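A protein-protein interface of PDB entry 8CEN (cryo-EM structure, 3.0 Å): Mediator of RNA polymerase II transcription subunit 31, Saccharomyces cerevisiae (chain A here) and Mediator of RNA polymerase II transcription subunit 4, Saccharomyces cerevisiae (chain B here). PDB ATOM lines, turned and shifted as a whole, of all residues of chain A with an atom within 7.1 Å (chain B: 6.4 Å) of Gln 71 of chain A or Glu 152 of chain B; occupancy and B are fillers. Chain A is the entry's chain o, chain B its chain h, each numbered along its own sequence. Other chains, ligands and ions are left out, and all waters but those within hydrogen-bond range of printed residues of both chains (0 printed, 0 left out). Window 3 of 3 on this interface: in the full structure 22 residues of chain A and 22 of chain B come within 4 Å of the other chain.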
ATOM      1  N   TRP A  64      -4.996  10.805 -30.996  1.00  0.00           N
ATOM      2  CA  TRP A  64      -4.534  12.089 -30.485  1.00  0.00           C
ATOM      3  C   TRP A  64      -5.339  13.255 -31.040  1.00  0.00           C
ATOM      4  O   TRP A  64      -5.233  14.368 -30.515  1.00  0.00           O
ATOM      5  CB  TRP A  64      -3.054  12.275 -30.817  1.00  0.00           C
ATOM      6  CG  TRP A  64      -2.155  11.354 -30.063  1.00  0.00           C
ATOM      7  CD1 TRP A  64      -1.422  10.327 -30.577  1.00  0.00           C
ATOM      8  CD2 TRP A  64      -1.897  11.366 -28.655  1.00  0.00           C
ATOM      9  NE1 TRP A  64      -0.719   9.702 -29.579  1.00  0.00           N
ATOM     10  CE2 TRP A  64      -0.996  10.320 -28.388  1.00  0.00           C
ATOM     11  CE3 TRP A  64      -2.339  12.162 -27.594  1.00  0.00           C
ATOM     12  CZ2 TRP A  64      -0.533  10.045 -27.107  1.00  0.00           C
ATOM     13  CZ3 TRP A  64      -1.877  11.887 -26.323  1.00  0.00           C
ATOM     14  CH2 TRP A  64      -0.981  10.839 -26.091  1.00  0.00           C
ATOM     15  N   CYS A  65      -6.117  13.024 -32.101  1.00  0.00           N
ATOM     16  CA  CYS A  65      -7.038  14.034 -32.610  1.00  0.00           C
ATOM     17  C   CYS A  65      -8.105  14.391 -31.585  1.00  0.00           C
ATOM     18  O   CYS A  65      -8.457  15.566 -31.428  1.00  0.00           O
ATOM     19  CB  CYS A  65      -7.689  13.524 -33.897  1.00  0.00           C
ATOM     20  SG  CYS A  65      -8.868  14.642 -34.669  1.00  0.00           S
ATOM     21  N   ASN A  66      -8.620  13.410 -30.885  1.00  0.00           N
ATOM     22  CA  ASN A  66      -9.804  13.614 -30.072  1.00  0.00           C
ATOM     23  C   ASN A  66      -9.441  13.801 -28.603  1.00  0.00           C
ATOM     24  O   ASN A  66      -8.424  13.282 -28.135  1.00  0.00           O
ATOM     25  CB  ASN A  66     -10.749  12.418 -30.216  1.00  0.00           C
ATOM     26  CG  ASN A  66     -11.268  12.257 -31.629  1.00  0.00           C
ATOM     27  OD1 ASN A  66     -10.968  11.272 -32.305  1.00  0.00           O
ATOM     28  ND2 ASN A  66     -12.045  13.231 -32.089  1.00  0.00           N
ATOM     29  N   PRO A  67     -10.255  14.552 -27.854  1.00  0.00           N
ATOM     30  CA  PRO A  67     -10.039  14.642 -26.411  1.00  0.00           C
ATOM     31  C   PRO A  67     -10.391  13.332 -25.737  1.00  0.00           C
ATOM     32  O   PRO A  67     -11.196  12.543 -26.265  1.00  0.00           O
ATOM     33  CB  PRO A  67     -10.993  15.773 -25.984  1.00  0.00           C
ATOM     34  CG  PRO A  67     -12.043  15.788 -27.033  1.00  0.00           C
ATOM     35  CD  PRO A  67     -11.325  15.458 -28.306  1.00  0.00           C
ATOM     36  N   PRO A  68      -9.817  13.044 -24.553  1.00  0.00           N
ATOM     37  CA  PRO A  68      -8.928  13.860 -23.717  1.00  0.00           C
ATOM     38  C   PRO A  68      -7.467  13.784 -24.135  1.00  0.00           C
ATOM     39  O   PRO A  68      -6.609  14.390 -23.496  1.00  0.00           O
ATOM     40  CB  PRO A  68      -9.118  13.249 -22.333  1.00  0.00           C
ATOM     41  CG  PRO A  68      -9.322  11.807 -22.624  1.00  0.00           C
ATOM     42  CD  PRO A  68     -10.102  11.747 -23.917  1.00  0.00           C
ATOM     43  N   TYR A  69      -7.199  13.026 -25.200  1.00  0.00           N
ATOM     44  CA  TYR A  69      -5.830  12.870 -25.678  1.00  0.00           C
ATOM     45  C   TYR A  69      -5.303  14.162 -26.283  1.00  0.00           C
ATOM     46  O   TYR A  69      -4.115  14.478 -26.152  1.00  0.00           O
ATOM     47  CB  TYR A  69      -5.771  11.735 -26.696  1.00  0.00           C
ATOM     48  CG  TYR A  69      -6.091  10.392 -26.100  1.00  0.00           C
ATOM     49  CD1 TYR A  69      -5.234   9.800 -25.186  1.00  0.00           C
ATOM     50  CD2 TYR A  69      -7.259   9.724 -26.435  1.00  0.00           C
ATOM     51  CE1 TYR A  69      -5.524   8.577 -24.633  1.00  0.00           C
ATOM     52  CE2 TYR A  69      -7.559   8.495 -25.887  1.00  0.00           C
ATOM     53  CZ  TYR A  69      -6.687   7.926 -24.986  1.00  0.00           C
ATOM     54  OH  TYR A  69      -6.979   6.702 -24.433  1.00  0.00           O
ATOM     55  N   SER A  70      -6.174  14.925 -26.945  1.00  0.00           N
ATOM     56  CA  SER A  70      -5.750  16.151 -27.607  1.00  0.00           C
ATOM     57  C   SER A  70      -5.400  17.259 -26.622  1.00  0.00           C
ATOM     58  O   SER A  70      -4.721  18.216 -27.007  1.00  0.00           O
ATOM     59  CB  SER A  70      -6.844  16.625 -28.561  1.00  0.00           C
ATOM     60  OG  SER A  70      -6.348  17.613 -29.440  1.00  0.00           O
ATOM     61  N   GLN A  71      -5.855  17.156 -25.368  1.00  0.00           N
ATOM     62  CA  GLN A  71      -5.494  18.142 -24.355  1.00  0.00           C
ATOM     63  C   GLN A  71      -4.007  18.103 -24.033  1.00  0.00           C
ATOM     64  O   GLN A  71      -3.413  19.141 -23.722  1.00  0.00           O
ATOM     65  CB  GLN A  71      -6.304  17.913 -23.079  1.00  0.00           C
ATOM     66  CG  GLN A  71      -7.782  17.654 -23.299  1.00  0.00           C
ATOM     67  CD  GLN A  71      -8.466  18.771 -24.057  1.00  0.00           C
ATOM     68  OE1 GLN A  71      -9.017  18.561 -25.136  1.00  0.00           O
ATOM     69  NE2 GLN A  71      -8.427  19.972 -23.496  1.00  0.00           N
ATOM     70  N   CYS A  72      -3.393  16.924 -24.095  1.00  0.00           N
ATOM     71  CA  CYS A  72      -1.988  16.770 -23.746  1.00  0.00           C
ATOM     72  C   CYS A  72      -1.043  17.106 -24.892  1.00  0.00           C
ATOM     73  O   CYS A  72       0.176  17.045 -24.701  1.00  0.00           O
ATOM     74  CB  CYS A  72      -1.723  15.342 -23.263  1.00  0.00           C
ATOM     75  SG  CYS A  72      -2.599  14.889 -21.751  1.00  0.00           S
ATOM     76  N   ILE A  73      -1.563  17.453 -26.066  1.00  0.00           N
ATOM     77  CA  ILE A  73      -0.719  17.792 -27.207  1.00  0.00           C
ATOM     78  C   ILE A  73      -0.182  19.204 -27.001  1.00  0.00           C
ATOM     79  O   ILE A  73      -0.930  20.182 -27.065  1.00  0.00           O
ATOM     80  CB  ILE A  73      -1.479  17.676 -28.531  1.00  0.00           C
ATOM     81  CG1 ILE A  73      -1.977  16.244 -28.733  1.00  0.00           C
ATOM     82  CG2 ILE A  73      -0.589  18.097 -29.682  1.00  0.00           C
ATOM     83  CD1 ILE A  73      -0.865  15.234 -28.905  1.00  0.00           C
ATOM     84  N   VAL A  74       1.122  19.309 -26.761  1.00  0.00           N
ATOM     85  CA  VAL A  74       1.749  20.602 -26.520  1.00  0.00           C
ATOM     86  C   VAL A  74       2.088  21.295 -27.836  1.00  0.00           C
ATOM     87  O   VAL A  74       2.017  22.526 -27.933  1.00  0.00           O
ATOM     88  CB  VAL A  74       2.989  20.383 -25.633  1.00  0.00           C
ATOM     89  CG1 VAL A  74       3.759  21.662 -25.414  1.00  0.00           C
ATOM     90  CG2 VAL A  74       2.572  19.770 -24.308  1.00  0.00           C
ATOM     91  N   ASN B 149     -15.941  22.590 -25.417  1.00  0.00           N
ATOM     92  CA  ASN B 149     -16.279  22.763 -24.011  1.00  0.00           C
ATOM     93  C   ASN B 149     -15.482  23.940 -23.464  1.00  0.00           C
ATOM     94  O   ASN B 149     -14.319  24.127 -23.830  1.00  0.00           O
ATOM     95  CB  ASN B 149     -15.969  21.488 -23.217  1.00  0.00           C
ATOM     96  CG  ASN B 149     -16.539  21.513 -21.809  1.00  0.00           C
ATOM     97  OD1 ASN B 149     -17.180  22.478 -21.395  1.00  0.00           O
ATOM     98  ND2 ASN B 149     -16.301  20.441 -21.062  1.00  0.00           N
ATOM     99  N   SER B 150     -16.109  24.733 -22.590  1.00  0.00           N
ATOM    100  CA  SER B 150     -15.492  25.981 -22.142  1.00  0.00           C
ATOM    101  C   SER B 150     -14.286  25.727 -21.243  1.00  0.00           C
ATOM    102  O   SER B 150     -13.222  26.328 -21.434  1.00  0.00           O
ATOM    103  CB  SER B 150     -16.523  26.847 -21.420  1.00  0.00           C
ATOM    104  OG  SER B 150     -16.948  26.235 -20.214  1.00  0.00           O
ATOM    105  N   THR B 151     -14.428  24.837 -20.257  1.00  0.00           N
ATOM    106  CA  THR B 151     -13.330  24.612 -19.321  1.00  0.00           C
ATOM    107  C   THR B 151     -12.191  23.824 -19.967  1.00  0.00           C
ATOM    108  O   THR B 151     -11.015  24.107 -19.707  1.00  0.00           O
ATOM    109  CB  THR B 151     -13.849  23.931 -18.045  1.00  0.00           C
ATOM    110  OG1 THR B 151     -12.772  23.763 -17.112  1.00  0.00           O
ATOM    111  CG2 THR B 151     -14.528  22.590 -18.326  1.00  0.00           C
ATOM    112  N   GLU B 152     -12.517  22.862 -20.838  1.00  0.00           N
ATOM    113  CA  GLU B 152     -11.486  22.158 -21.594  1.00  0.00           C
ATOM    114  C   GLU B 152     -10.775  23.105 -22.551  1.00  0.00           C
ATOM    115  O   GLU B 152      -9.553  23.024 -22.724  1.00  0.00           O
ATOM    116  CB  GLU B 152     -12.106  20.989 -22.356  1.00  0.00           C
ATOM    117  CG  GLU B 152     -12.748  19.939 -21.465  1.00  0.00           C
ATOM    118  CD  GLU B 152     -13.129  18.683 -22.224  1.00  0.00           C
ATOM    119  OE1 GLU B 152     -12.283  18.164 -22.983  1.00  0.00           O
ATOM    120  OE2 GLU B 152     -14.276  18.214 -22.062  1.00  0.00           O
ATOM    121  N   LEU B 153     -11.536  24.019 -23.160  1.00  0.00           N
ATOM    122  CA  LEU B 153     -10.982  25.058 -24.018  1.00  0.00           C
ATOM    123  C   LEU B 153      -9.984  25.924 -23.265  1.00  0.00           C
ATOM    124  O   LEU B 153      -8.867  26.158 -23.738  1.00  0.00           O
ATOM    125  CB  LEU B 153     -12.127  25.915 -24.554  1.00  0.00           C
ATOM    126  CG  LEU B 153     -11.888  27.147 -25.420  1.00  0.00           C
ATOM    127  CD1 LEU B 153     -12.963  27.163 -26.455  1.00  0.00           C
ATOM    128  CD2 LEU B 153     -11.941  28.433 -24.610  1.00  0.00           C
ATOM    129  N   LEU B 154     -10.380  26.410 -22.087  1.00  0.00           N
ATOM    130  CA  LEU B 154      -9.516  27.301 -21.322  1.00  0.00           C
ATOM    131  C   LEU B 154      -8.279  26.576 -20.809  1.00  0.00           C
ATOM    132  O   LEU B 154      -7.178  27.138 -20.831  1.00  0.00           O
ATOM    133  CB  LEU B 154     -10.300  27.927 -20.170  1.00  0.00           C
ATOM    134  CG  LEU B 154     -11.269  29.036 -20.585  1.00  0.00           C
ATOM    135  CD1 LEU B 154     -12.260  29.336 -19.474  1.00  0.00           C
ATOM    136  CD2 LEU B 154     -10.508  30.293 -20.982  1.00  0.00           C
ATOM    137  N   ASP B 155      -8.433  25.322 -20.366  1.00  0.00           N
ATOM    138  CA  ASP B 155      -7.284  24.551 -19.900  1.00  0.00           C
ATOM    139  C   ASP B 155      -6.303  24.263 -21.033  1.00  0.00           C
ATOM    140  O   ASP B 155      -5.087  24.419 -20.862  1.00  0.00           O
ATOM    141  CB  ASP B 155      -7.755  23.251 -19.253  1.00  0.00           C
ATOM    142  CG  ASP B 155      -8.482  23.484 -17.943  1.00  0.00           C
ATOM    143  OD1 ASP B 155      -8.172  24.484 -17.261  1.00  0.00           O
ATOM    144  OD2 ASP B 155      -9.364  22.670 -17.597  1.00  0.00           O
ATOM    145  N   TYR B 156      -6.808  23.873 -22.206  1.00  0.00           N
ATOM    146  CA  TYR B 156      -5.919  23.596 -23.328  1.00  0.00           C
ATOM    147  C   TYR B 156      -5.250  24.870 -23.831  1.00  0.00           C
ATOM    148  O   TYR B 156      -4.070  24.855 -24.201  1.00  0.00           O
ATOM    149  CB  TYR B 156      -6.690  22.913 -24.452  1.00  0.00           C
ATOM    150  CG  TYR B 156      -5.797  22.400 -25.550  1.00  0.00           C
ATOM    151  CD1 TYR B 156      -4.607  21.754 -25.252  1.00  0.00           C
ATOM    152  CD2 TYR B 156      -6.137  22.567 -26.883  1.00  0.00           C
ATOM    153  CE1 TYR B 156      -3.784  21.284 -26.248  1.00  0.00           C
ATOM    154  CE2 TYR B 156      -5.320  22.100 -27.885  1.00  0.00           C
ATOM    155  CZ  TYR B 156      -4.144  21.459 -27.565  1.00  0.00           C
ATOM    156  OH  TYR B 156      -3.323  20.992 -28.565  1.00  0.00           O
ATOM    157  N   ALA B 157      -5.979  25.985 -23.828  1.00  0.00           N
ATOM    158  CA  ALA B 157      -5.409  27.237 -24.310  1.00  0.00           C
ATOM    159  C   ALA B 157      -4.364  27.786 -23.343  1.00  0.00           C
ATOM    160  O   ALA B 157      -3.338  28.326 -23.775  1.00  0.00           O
ATOM    161  CB  ALA B 157      -6.529  28.244 -24.553  1.00  0.00           C
ATOM    162  N   LYS B 159      -2.581  25.830 -21.520  1.00  0.00           N
ATOM    163  CA  LYS B 159      -1.441  24.953 -21.776  1.00  0.00           C
ATOM    164  C   LYS B 159      -0.628  25.449 -22.966  1.00  0.00           C
ATOM    165  O   LYS B 159       0.607  25.495 -22.913  1.00  0.00           O
ATOM    166  CB  LYS B 159      -1.915  23.522 -22.016  1.00  0.00           C
ATOM    167  CG  LYS B 159      -2.232  22.748 -20.758  1.00  0.00           C
ATOM    168  CD  LYS B 159      -2.459  21.284 -21.072  1.00  0.00           C
ATOM    169  CE  LYS B 159      -3.003  20.545 -19.866  1.00  0.00           C
ATOM    170  NZ  LYS B 159      -3.242  19.104 -20.162  1.00  0.00           N
ATOM    171  N   LEU B 160      -1.308  25.829 -24.050  1.00  0.00           N
ATOM    172  CA  LEU B 160      -0.628  26.259 -25.267  1.00  0.00           C
ATOM    173  C   LEU B 160      -0.134  27.699 -25.218  1.00  0.00           C
ATOM    174  O   LEU B 160       0.502  28.139 -26.183  1.00  0.00           O
ATOM    175  CB  LEU B 160      -1.548  26.106 -26.478  1.00  0.00           C
ATOM    176  CG  LEU B 160      -2.079  24.717 -26.812  1.00  0.00           C
ATOM    177  CD1 LEU B 160      -2.981  24.805 -28.025  1.00  0.00           C
ATOM    178  CD2 LEU B 160      -0.940  23.748 -27.052  1.00  0.00           C
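The backbone carbonyl oxygen of Ser 70 of chain A lies close to the side-chain hydroxyl of Tyr 156 of chain B, 3.5 Å away.
The backbone carbonyl oxygen (O) of Ile 73 of chain A is in hydrogen-bond range of the side-chain hydroxyl (OH) of Tyr 156 of chain B (2.9 Å).
The backbone carbonyl oxygen (O) of Glu 152 of chain B is in hydrogen-bond range of the side-chain amide nitrogen (NE2) of Gln 71 of chain A (3.3 Å).
Of the 11 printed residues of chain B, 4 touch a printed residue of chain A.
Hydrophobic or aromatic side chains of chain B that line the printed part of chain A: Tyr 156 and Leu 160.
Printed residues of chain A that touch a printed residue of chain B: Ser 70, Gln 71, Ile 73 and Val 74.
Hydrophobic or aromatic side chains of chain A within 4 Å of the printed part of chain B: Ile 73.
Among the printed residues, no Asp or Glu carboxylate lies within 4 Å of a Lys or Arg side-chain nitrogen of the other chain.
Gln 71 of chain A touches Tyr 156 of chain B.
Gln 71 of chain A touches Lys 159 of chain B.
CD2 of Leu 160 of chain B touches O of Ile 73 of chain A (3.6 Å).
Val 74 of chain A touches Leu 160 of chain B.
The side-chain carboxylate of Glu 152 of chain B sits at hydrogen-bond distance from the side-chain amide nitrogen of Asn 149 of chain B, at 3.2 Å.
Printed residues of chain B within 4 Å of Ser 70 of chain A: Tyr 156 (3.3 Å).
Gln 71 of chain A touches just these residues of chain B: Glu 152, Tyr 156 and Lys 159.
Of the printed residues of chain B, Val 74 of chain A touches Leu 160 (3.3 Å).
Asn 149 of chain B touches none of the printed residues of chain A.
Glu 152 of chain B touches just one residue of chain A: Gln 71 (3.3 Å).
The nearest residue of chain B that does not touch Gln 71 of chain A is Leu 153 of chain B (5.1 Å).
The nearest residue of chain A that does not touch Glu 152 of chain B is Pro 67 of chain A (4.05 Å).
The nearest printed residue of chain B that does not touch Ser 70 of chain A is Leu 160 of chain B (6.7 Å).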
